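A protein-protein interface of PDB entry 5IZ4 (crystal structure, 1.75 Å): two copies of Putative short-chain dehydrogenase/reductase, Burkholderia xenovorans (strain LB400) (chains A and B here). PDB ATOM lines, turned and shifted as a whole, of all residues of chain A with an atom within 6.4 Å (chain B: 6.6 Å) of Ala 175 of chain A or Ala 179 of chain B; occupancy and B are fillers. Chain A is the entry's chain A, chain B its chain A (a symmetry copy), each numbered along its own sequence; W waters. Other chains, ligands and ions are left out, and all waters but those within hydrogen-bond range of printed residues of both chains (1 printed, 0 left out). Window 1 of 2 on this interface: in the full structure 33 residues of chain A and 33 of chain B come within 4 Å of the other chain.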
ATOM      1  N   PHE A 121      18.999  28.951   7.261  1.00  0.00           N
ATOM      2  CA  PHE A 121      19.315  27.621   7.773  1.00  0.00           C
ATOM      3  C   PHE A 121      20.801  27.522   8.087  1.00  0.00           C
ATOM      4  O   PHE A 121      21.191  27.037   9.156  1.00  0.00           O
ATOM      5  CB  PHE A 121      18.924  26.530   6.765  1.00  0.00           C
ATOM      6  CG  PHE A 121      17.469  26.112   6.807  1.00  0.00           C
ATOM      7  CD1 PHE A 121      16.538  26.701   5.959  1.00  0.00           C
ATOM      8  CD2 PHE A 121      17.042  25.105   7.663  1.00  0.00           C
ATOM      9  CE1 PHE A 121      15.213  26.309   5.967  1.00  0.00           C
ATOM     10  CE2 PHE A 121      15.704  24.703   7.679  1.00  0.00           C
ATOM     11  CZ  PHE A 121      14.790  25.308   6.834  1.00  0.00           C
ATOM     12  N   TYR A 125      22.684  27.256  11.789  1.00  0.00           N
ATOM     13  CA  TYR A 125      23.450  26.029  11.977  1.00  0.00           C
ATOM     14  C   TYR A 125      24.906  26.338  12.278  1.00  0.00           C
ATOM     15  O   TYR A 125      25.561  25.602  13.028  1.00  0.00           O
ATOM     16  CB  TYR A 125      23.344  25.170  10.722  1.00  0.00           C
ATOM     17  CG  TYR A 125      23.694  23.706  10.863  1.00  0.00           C
ATOM     18  CD1 TYR A 125      24.817  23.179  10.238  1.00  0.00           C
ATOM     19  CD2 TYR A 125      22.870  22.836  11.572  1.00  0.00           C
ATOM     20  CE1 TYR A 125      25.124  21.817  10.326  1.00  0.00           C
ATOM     21  CE2 TYR A 125      23.163  21.496  11.667  1.00  0.00           C
ATOM     22  CZ  TYR A 125      24.293  20.985  11.051  1.00  0.00           C
ATOM     23  OH  TYR A 125      24.577  19.622  11.136  1.00  0.00           O
ATOM     24  N   ALA A 162      12.639  22.945  21.249  1.00  0.00           N
ATOM     25  CA  ALA A 162      12.410  22.950  19.805  1.00  0.00           C
ATOM     26  C   ALA A 162      13.098  21.779  19.110  1.00  0.00           C
ATOM     27  O   ALA A 162      12.586  21.272  18.104  1.00  0.00           O
ATOM     28  CB  ALA A 162      12.894  24.276  19.194  1.00  0.00           C
ATOM     29  N   GLY A 163      14.274  21.365  19.593  1.00  0.00           N
ATOM     30  CA  GLY A 163      14.955  20.239  18.975  1.00  0.00           C
ATOM     31  C   GLY A 163      14.222  18.932  19.192  1.00  0.00           C
ATOM     32  O   GLY A 163      14.321  18.013  18.373  1.00  0.00           O
ATOM     33  N   SER A 170      11.947  29.169  14.889  1.00  0.00           N
ATOM     34  CA  SER A 170      11.877  28.935  13.451  1.00  0.00           C
ATOM     35  C   SER A 170      12.187  27.476  13.174  1.00  0.00           C
ATOM     36  O   SER A 170      12.761  26.777  14.010  1.00  0.00           O
ATOM     37  CB  SER A 170      12.860  29.812  12.669  1.00  0.00           C
ATOM     38  OG  SER A 170      14.176  29.265  12.716  1.00  0.00           O
ATOM     39  N   ILE A 171      11.822  27.031  11.972  1.00  0.00           N
ATOM     40  CA  ILE A 171      12.126  25.654  11.603  1.00  0.00           C
ATOM     41  C   ILE A 171      13.633  25.461  11.434  1.00  0.00           C
ATOM     42  O   ILE A 171      14.154  24.362  11.674  1.00  0.00           O
ATOM     43  CB  ILE A 171      11.334  25.259  10.339  1.00  0.00           C
ATOM     44  CG1 ILE A 171      11.331  23.734  10.164  1.00  0.00           C
ATOM     45  CG2 ILE A 171      11.876  25.966   9.089  1.00  0.00           C
ATOM     46  CD1 ILE A 171      10.580  23.260   8.927  1.00  0.00           C
ATOM     47  N   ALA A 172      14.363  26.515  11.032  1.00  0.00           N
ATOM     48  CA  ALA A 172      15.820  26.410  10.962  1.00  0.00           C
ATOM     49  C   ALA A 172      16.426  26.268  12.351  1.00  0.00           C
ATOM     50  O   ALA A 172      17.401  25.529  12.545  1.00  0.00           O
ATOM     51  CB  ALA A 172      16.411  27.631  10.240  1.00  0.00           C
ATOM     52  N   TYR A 173      15.863  26.972  13.332  1.00  0.00           N
ATOM     53  CA  TYR A 173      16.323  26.827  14.708  1.00  0.00           C
ATOM     54  C   TYR A 173      16.025  25.427  15.228  1.00  0.00           C
ATOM     55  O   TYR A 173      16.895  24.760  15.806  1.00  0.00           O
ATOM     56  CB  TYR A 173      15.649  27.891  15.580  1.00  0.00           C
ATOM     57  CG  TYR A 173      16.009  27.842  17.042  1.00  0.00           C
ATOM     58  CD1 TYR A 173      17.152  28.470  17.521  1.00  0.00           C
ATOM     59  CD2 TYR A 173      15.194  27.178  17.952  1.00  0.00           C
ATOM     60  CE1 TYR A 173      17.475  28.444  18.871  1.00  0.00           C
ATOM     61  CE2 TYR A 173      15.507  27.141  19.302  1.00  0.00           C
ATOM     62  CZ  TYR A 173      16.652  27.774  19.754  1.00  0.00           C
ATOM     63  OH  TYR A 173      16.971  27.740  21.094  1.00  0.00           O
ATOM     64  N   ALA A 174      14.806  24.948  15.002  1.00  0.00           N
ATOM     65  CA  ALA A 174      14.446  23.619  15.488  1.00  0.00           C
ATOM     66  C   ALA A 174      15.361  22.559  14.883  1.00  0.00           C
ATOM     67  O   ALA A 174      15.865  21.679  15.592  1.00  0.00           O
ATOM     68  CB  ALA A 174      12.985  23.324  15.162  1.00  0.00           C
ATOM     69  N   ALA A 175      15.590  22.637  13.569  1.00  0.00           N
ATOM     70  CA  ALA A 175      16.472  21.679  12.912  1.00  0.00           C
ATOM     71  C   ALA A 175      17.863  21.707  13.527  1.00  0.00           C
ATOM     72  O   ALA A 175      18.460  20.651  13.781  1.00  0.00           O
ATOM     73  CB  ALA A 175      16.550  21.967  11.412  1.00  0.00           C
ATOM     74  N   SER A 176      18.395  22.908  13.782  1.00  0.00           N
ATOM     75  CA  SER A 176      19.750  22.994  14.315  1.00  0.00           C
ATOM     76  C   SER A 176      19.829  22.367  15.692  1.00  0.00           C
ATOM     77  O   SER A 176      20.860  21.783  16.045  1.00  0.00           O
ATOM     78  CB  SER A 176      20.235  24.458  14.351  1.00  0.00           C
ATOM     79  OG  SER A 176      19.611  25.172  15.417  1.00  0.00           O
ATOM     80  N   LYS A 177      18.737  22.424  16.461  1.00  0.00           N
ATOM     81  CA  LYS A 177      18.756  21.867  17.810  1.00  0.00           C
ATOM     82  C   LYS A 177      18.530  20.358  17.794  1.00  0.00           C
ATOM     83  O   LYS A 177      19.054  19.638  18.661  1.00  0.00           O
ATOM     84  CB  LYS A 177      17.719  22.588  18.672  1.00  0.00           C
ATOM     85  CG  LYS A 177      18.035  24.065  18.895  1.00  0.00           C
ATOM     86  CD  LYS A 177      19.365  24.281  19.618  1.00  0.00           C
ATOM     87  CE  LYS A 177      19.486  25.731  20.090  1.00  0.00           C
ATOM     88  NZ  LYS A 177      20.721  25.983  20.915  1.00  0.00           N
ATOM     89  N   GLY A 178      17.789  19.846  16.808  1.00  0.00           N
ATOM     90  CA  GLY A 178      17.768  18.407  16.618  1.00  0.00           C
ATOM     91  C   GLY A 178      19.152  17.868  16.310  1.00  0.00           C
ATOM     92  O   GLY A 178      19.543  16.803  16.796  1.00  0.00           O
ATOM     93  N   ALA A 179      19.918  18.605  15.503  1.00  0.00           N
ATOM     94  CA  ALA A 179      21.294  18.209  15.229  1.00  0.00           C
ATOM     95  C   ALA A 179      22.142  18.255  16.497  1.00  0.00           C
ATOM     96  O   ALA A 179      22.993  17.383  16.711  1.00  0.00           O
ATOM     97  CB  ALA A 179      21.889  19.120  14.151  1.00  0.00           C
ATOM     98  N   VAL A 180      21.937  19.272  17.341  1.00  0.00           N
ATOM     99  CA  VAL A 180      22.682  19.347  18.600  1.00  0.00           C
ATOM    100  C   VAL A 180      22.395  18.115  19.453  1.00  0.00           C
ATOM    101  O   VAL A 180      23.304  17.523  20.051  1.00  0.00           O
ATOM    102  CB  VAL A 180      22.352  20.646  19.362  1.00  0.00           C
ATOM    103  CG1 VAL A 180      22.917  20.585  20.784  1.00  0.00           C
ATOM    104  CG2 VAL A 180      22.926  21.867  18.620  1.00  0.00           C
ATOM    105  N   THR A 182      21.523  15.056  18.494  1.00  0.00           N
ATOM    106  CA  THR A 182      22.227  13.893  17.957  1.00  0.00           C
ATOM    107  C   THR A 182      23.733  14.027  18.127  1.00  0.00           C
ATOM    108  O   THR A 182      24.422  13.044  18.436  1.00  0.00           O
ATOM    109  CB  THR A 182      21.887  13.717  16.478  1.00  0.00           C
ATOM    110  OG1 THR A 182      20.472  13.546  16.338  1.00  0.00           O
ATOM    111  CG2 THR A 182      22.606  12.508  15.899  1.00  0.00           C
ATOM    112  N   TYR B 125      24.939  19.011   5.252  1.00  0.00           N
ATOM    113  CA  TYR B 125      23.683  19.635   5.655  1.00  0.00           C
ATOM    114  C   TYR B 125      22.968  20.238   4.458  1.00  0.00           C
ATOM    115  O   TYR B 125      21.731  20.256   4.412  1.00  0.00           O
ATOM    116  CB  TYR B 125      23.967  20.713   6.696  1.00  0.00           C
ATOM    117  CG  TYR B 125      22.801  21.171   7.541  1.00  0.00           C
ATOM    118  CD1 TYR B 125      22.296  22.460   7.419  1.00  0.00           C
ATOM    119  CD2 TYR B 125      22.242  20.336   8.504  1.00  0.00           C
ATOM    120  CE1 TYR B 125      21.247  22.906   8.228  1.00  0.00           C
ATOM    121  CE2 TYR B 125      21.208  20.765   9.304  1.00  0.00           C
ATOM    122  CZ  TYR B 125      20.704  22.047   9.164  1.00  0.00           C
ATOM    123  OH  TYR B 125      19.667  22.482   9.989  1.00  0.00           O
ATOM    124  N   LEU B 129      19.536  18.266   4.621  1.00  0.00           N
ATOM    125  CA  LEU B 129      18.540  19.015   5.371  1.00  0.00           C
ATOM    126  C   LEU B 129      17.997  20.181   4.562  1.00  0.00           C
ATOM    127  O   LEU B 129      16.787  20.237   4.321  1.00  0.00           O
ATOM    128  CB  LEU B 129      19.125  19.495   6.714  1.00  0.00           C
ATOM    129  CG  LEU B 129      18.161  20.098   7.744  1.00  0.00           C
ATOM    130  CD1 LEU B 129      17.691  21.511   7.354  1.00  0.00           C
ATOM    131  CD2 LEU B 129      16.973  19.164   7.979  1.00  0.00           C
ATOM    132  N   GLY B 163      20.732   9.358  12.700  1.00  0.00           N
ATOM    133  CA  GLY B 163      20.071  10.510  13.292  1.00  0.00           C
ATOM    134  C   GLY B 163      19.494  10.204  14.658  1.00  0.00           C
ATOM    135  O   GLY B 163      19.373  11.096  15.504  1.00  0.00           O
ATOM    136  N   ALA B 174      25.475  12.274  10.913  1.00  0.00           N
ATOM    137  CA  ALA B 174      24.536  12.003  11.997  1.00  0.00           C
ATOM    138  C   ALA B 174      23.792  13.274  12.395  1.00  0.00           C
ATOM    139  O   ALA B 174      22.566  13.264  12.560  1.00  0.00           O
ATOM    140  CB  ALA B 174      25.278  11.412  13.192  1.00  0.00           C
ATOM    141  N   ALA B 175      24.525  14.380  12.547  1.00  0.00           N
ATOM    142  CA  ALA B 175      23.892  15.646  12.903  1.00  0.00           C
ATOM    143  C   ALA B 175      22.844  16.040  11.873  1.00  0.00           C
ATOM    144  O   ALA B 175      21.739  16.471  12.233  1.00  0.00           O
ATOM    145  CB  ALA B 175      24.943  16.749  13.038  1.00  0.00           C
ATOM    146  N   SER B 176      23.168  15.893  10.583  1.00  0.00           N
ATOM    147  CA  SER B 176      22.224  16.314   9.554  1.00  0.00           C
ATOM    148  C   SER B 176      20.959  15.481   9.609  1.00  0.00           C
ATOM    149  O   SER B 176      19.871  15.993   9.327  1.00  0.00           O
ATOM    150  CB  SER B 176      22.868  16.240   8.154  1.00  0.00           C
ATOM    151  OG  SER B 176      22.972  14.886   7.715  1.00  0.00           O
ATOM    152  N   LYS B 177      21.071  14.216  10.026  1.00  0.00           N
ATOM    153  CA  LYS B 177      19.897  13.349  10.073  1.00  0.00           C
ATOM    154  C   LYS B 177      19.084  13.579  11.344  1.00  0.00           C
ATOM    155  O   LYS B 177      17.851  13.426  11.335  1.00  0.00           O
ATOM    156  CB  LYS B 177      20.335  11.891   9.935  1.00  0.00           C
ATOM    157  CG  LYS B 177      20.957  11.569   8.579  1.00  0.00           C
ATOM    158  CD  LYS B 177      19.990  11.801   7.417  1.00  0.00           C
ATOM    159  CE  LYS B 177      20.541  11.178   6.132  1.00  0.00           C
ATOM    160  NZ  LYS B 177      19.582  11.265   4.974  1.00  0.00           N
ATOM    161  N   GLY B 178      19.735  13.980  12.440  1.00  0.00           N
ATOM    162  CA  GLY B 178      18.970  14.451  13.580  1.00  0.00           C
ATOM    163  C   GLY B 178      18.135  15.666  13.224  1.00  0.00           C
ATOM    164  O   GLY B 178      16.985  15.797  13.655  1.00  0.00           O
ATOM    165  N   ALA B 179      18.701  16.569  12.421  1.00  0.00           N
ATOM    166  CA  ALA B 179      17.937  17.721  11.954  1.00  0.00           C
ATOM    167  C   ALA B 179      16.774  17.285  11.068  1.00  0.00           C
ATOM    168  O   ALA B 179      15.680  17.860  11.147  1.00  0.00           O
ATOM    169  CB  ALA B 179      18.861  18.680  11.197  1.00  0.00           C
ATOM    170  N   VAL B 180      16.993  16.285  10.207  1.00  0.00           N
ATOM    171  CA  VAL B 180      15.904  15.787   9.365  1.00  0.00           C
ATOM    172  C   VAL B 180      14.765  15.263  10.235  1.00  0.00           C
ATOM    173  O   VAL B 180      13.583  15.519   9.966  1.00  0.00           O
ATOM    174  CB  VAL B 180      16.409  14.704   8.391  1.00  0.00           C
ATOM    175  CG1 VAL B 180      15.226  14.004   7.715  1.00  0.00           C
ATOM    176  CG2 VAL B 180      17.331  15.326   7.324  1.00  0.00           C
ATOM    177  N   ASN B 181      15.104  14.531  11.296  1.00  0.00           N
ATOM    178  CA  ASN B 181      14.074  13.999  12.187  1.00  0.00           C
ATOM    179  C   ASN B 181      13.234  15.120  12.794  1.00  0.00           C
ATOM    180  O   ASN B 181      11.999  15.055  12.798  1.00  0.00           O
ATOM    181  CB  ASN B 181      14.726  13.146  13.274  1.00  0.00           C
ATOM    182  CG  ASN B 181      15.391  11.905  12.709  1.00  0.00           C
ATOM    183  OD1 ASN B 181      15.167  11.551  11.556  1.00  0.00           O
ATOM    184  ND2 ASN B 181      16.193  11.224  13.526  1.00  0.00           N
ATOM    185  N   THR B 182      13.887  16.167  13.309  1.00  0.00           N
ATOM    186  CA  THR B 182      13.143  17.280  13.894  1.00  0.00           C
ATOM    187  C   THR B 182      12.374  18.053  12.833  1.00  0.00           C
ATOM    188  O   THR B 182      11.235  18.482  13.069  1.00  0.00           O
ATOM    189  CB  THR B 182      14.102  18.218  14.625  1.00  0.00           C
ATOM    190  OG1 THR B 182      14.785  17.488  15.650  1.00  0.00           O
ATOM    191  CG2 THR B 182      13.348  19.383  15.247  1.00  0.00           C
ATOM    192  N   LEU B 183      13.001  18.284  11.677  1.00  0.00           N
ATOM    193  CA  LEU B 183      12.328  18.992  10.593  1.00  0.00           C
ATOM    194  C   LEU B 183      11.050  18.267  10.190  1.00  0.00           C
ATOM    195  O   LEU B 183      10.028  18.899   9.899  1.00  0.00           O
ATOM    196  CB  LEU B 183      13.264  19.122   9.388  1.00  0.00           C
ATOM    197  CG  LEU B 183      12.781  20.031   8.258  1.00  0.00           C
ATOM    198  CD1 LEU B 183      13.484  21.392   8.337  1.00  0.00           C
ATOM    199  CD2 LEU B 183      13.064  19.378   6.914  1.00  0.00           C
ATOM    200  N   THR B 184      11.104  16.938  10.169  1.00  0.00           N
ATOM    201  CA  THR B 184       9.925  16.135   9.875  1.00  0.00           C
ATOM    202  C   THR B 184       8.774  16.464  10.827  1.00  0.00           C
ATOM    203  O   THR B 184       7.616  16.548  10.403  1.00  0.00           O
ATOM    204  CB  THR B 184      10.308  14.660   9.941  1.00  0.00           C
ATOM    205  OG1 THR B 184      11.289  14.387   8.922  1.00  0.00           O
ATOM    206  CG2 THR B 184       9.098  13.762   9.743  1.00  0.00           C
HETATM  207  O   HOH W   1      19.406  25.163  10.532  1.00  0.00           O
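Leu 129 of chain B touches Phe 121 of chain A (CD1 to CD2, 3.7 Å). CE2 of Tyr 125 of chain B touches CE2 of Tyr 125 of chain A, at 3.2 Å. Leu 183 of chain B touches Ile 171 of chain A (CD1 to CD1, 3.5 Å). Ala 174 of chain A touches Thr 182 of chain B. Ala 175 of chain A touches Tyr 125 of chain B. Gly 178 of chain A touches Gly 178 of chain B. Gly 178 of chain A touches Thr 182 of chain B. Ala 175 of chain B touches Ala 179 of chain A (O to CB, 3.3 Å). Ala 179 of chain A touches Ala 179 of chain B (N to N, 3.9 Å). CG2 of Thr 182 of chain A touches O of Ala 174 of chain B, 3.4 Å away.
The side-chain hydroxyl of Thr 182 of chain A lies within hydrogen-bond range of the backbone carbonyl oxygen of Gly 178 of chain A (3.4 Å). O of Gly 178 of chain B lies within hydrogen-bond range of OG1 of Thr 182 of chain B, at 3.4 Å.
Of the printed residues of chain B, Ala 162 of chain A touches Thr 182 (3.5 Å). Ala 175 of chain A touches just these residues of chain B: Tyr 125 and Ala 179. Printed residues of chain B within 4 Å of Ala 179 of chain A: Ala 175 (3.3 Å) and Ala 179 (3.9 Å). Of the printed residues of chain A, Leu 129 of chain B touches Phe 121. Of the printed residues of chain A, Ala 174 of chain B touches Thr 182 (3.4 Å). Ala 179 of chain B touches two residues of chain A. The nearest residue of chain B that does not touch Ala 175 of chain A is Leu 129 of chain B (4.2 Å). The nearest printed residue of chain B that does not touch Tyr 125 of chain A is Ser 176 of chain B (4.02 Å).
Hydrophobic or aromatic side chains of chain B within 4 Å of the printed part of chain A: Tyr 125, Leu 129, Ala 174, Ala 175, Ala 179 and Leu 183. Among the printed residues, 16 pairs touch across the chains.
Tyr 125 of chain A touches its own counterpart, Tyr 125 of chain B. Gly 178 of chain A touches its own counterpart, Gly 178 of chain B. Gly 178 of chain A touches Thr 182 of chain B, and with the chains exchanged Thr 182 of chain A touches Gly 178 of chain B. Ala 179 of chain A touches its own counterpart, Ala 179 of chain B. Positions printed for both chains: 125, 163, 174, 175, 176, 177, 178, 179, 180 and 182. Of the 16 pairs that touch across the chains among the printed residues, 13 have their exchanged pair printed and touching as well.
The backbone carbonyl oxygen (O) of Gly 163 of chain A is in hydrogen-bond range of the side-chain hydroxyl (OG1) of Thr 182 of chain B (2.8 Å). The side-chain hydroxyl of Thr 182 of chain A sits at hydrogen-bond distance from the backbone carbonyl oxygen of Gly 163 of chain B, 2.8 Å away.
Water W1 lies within hydrogen-bond range of the side-chain hydroxyl (OH) of Tyr 125 of chain B (2.7 Å), the backbone carbonyl oxygen (O) of Ala 172 of chain A (2.9 Å) and the backbone carbonyl oxygen (O) of Phe 121 of chain A (2.9 Å).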
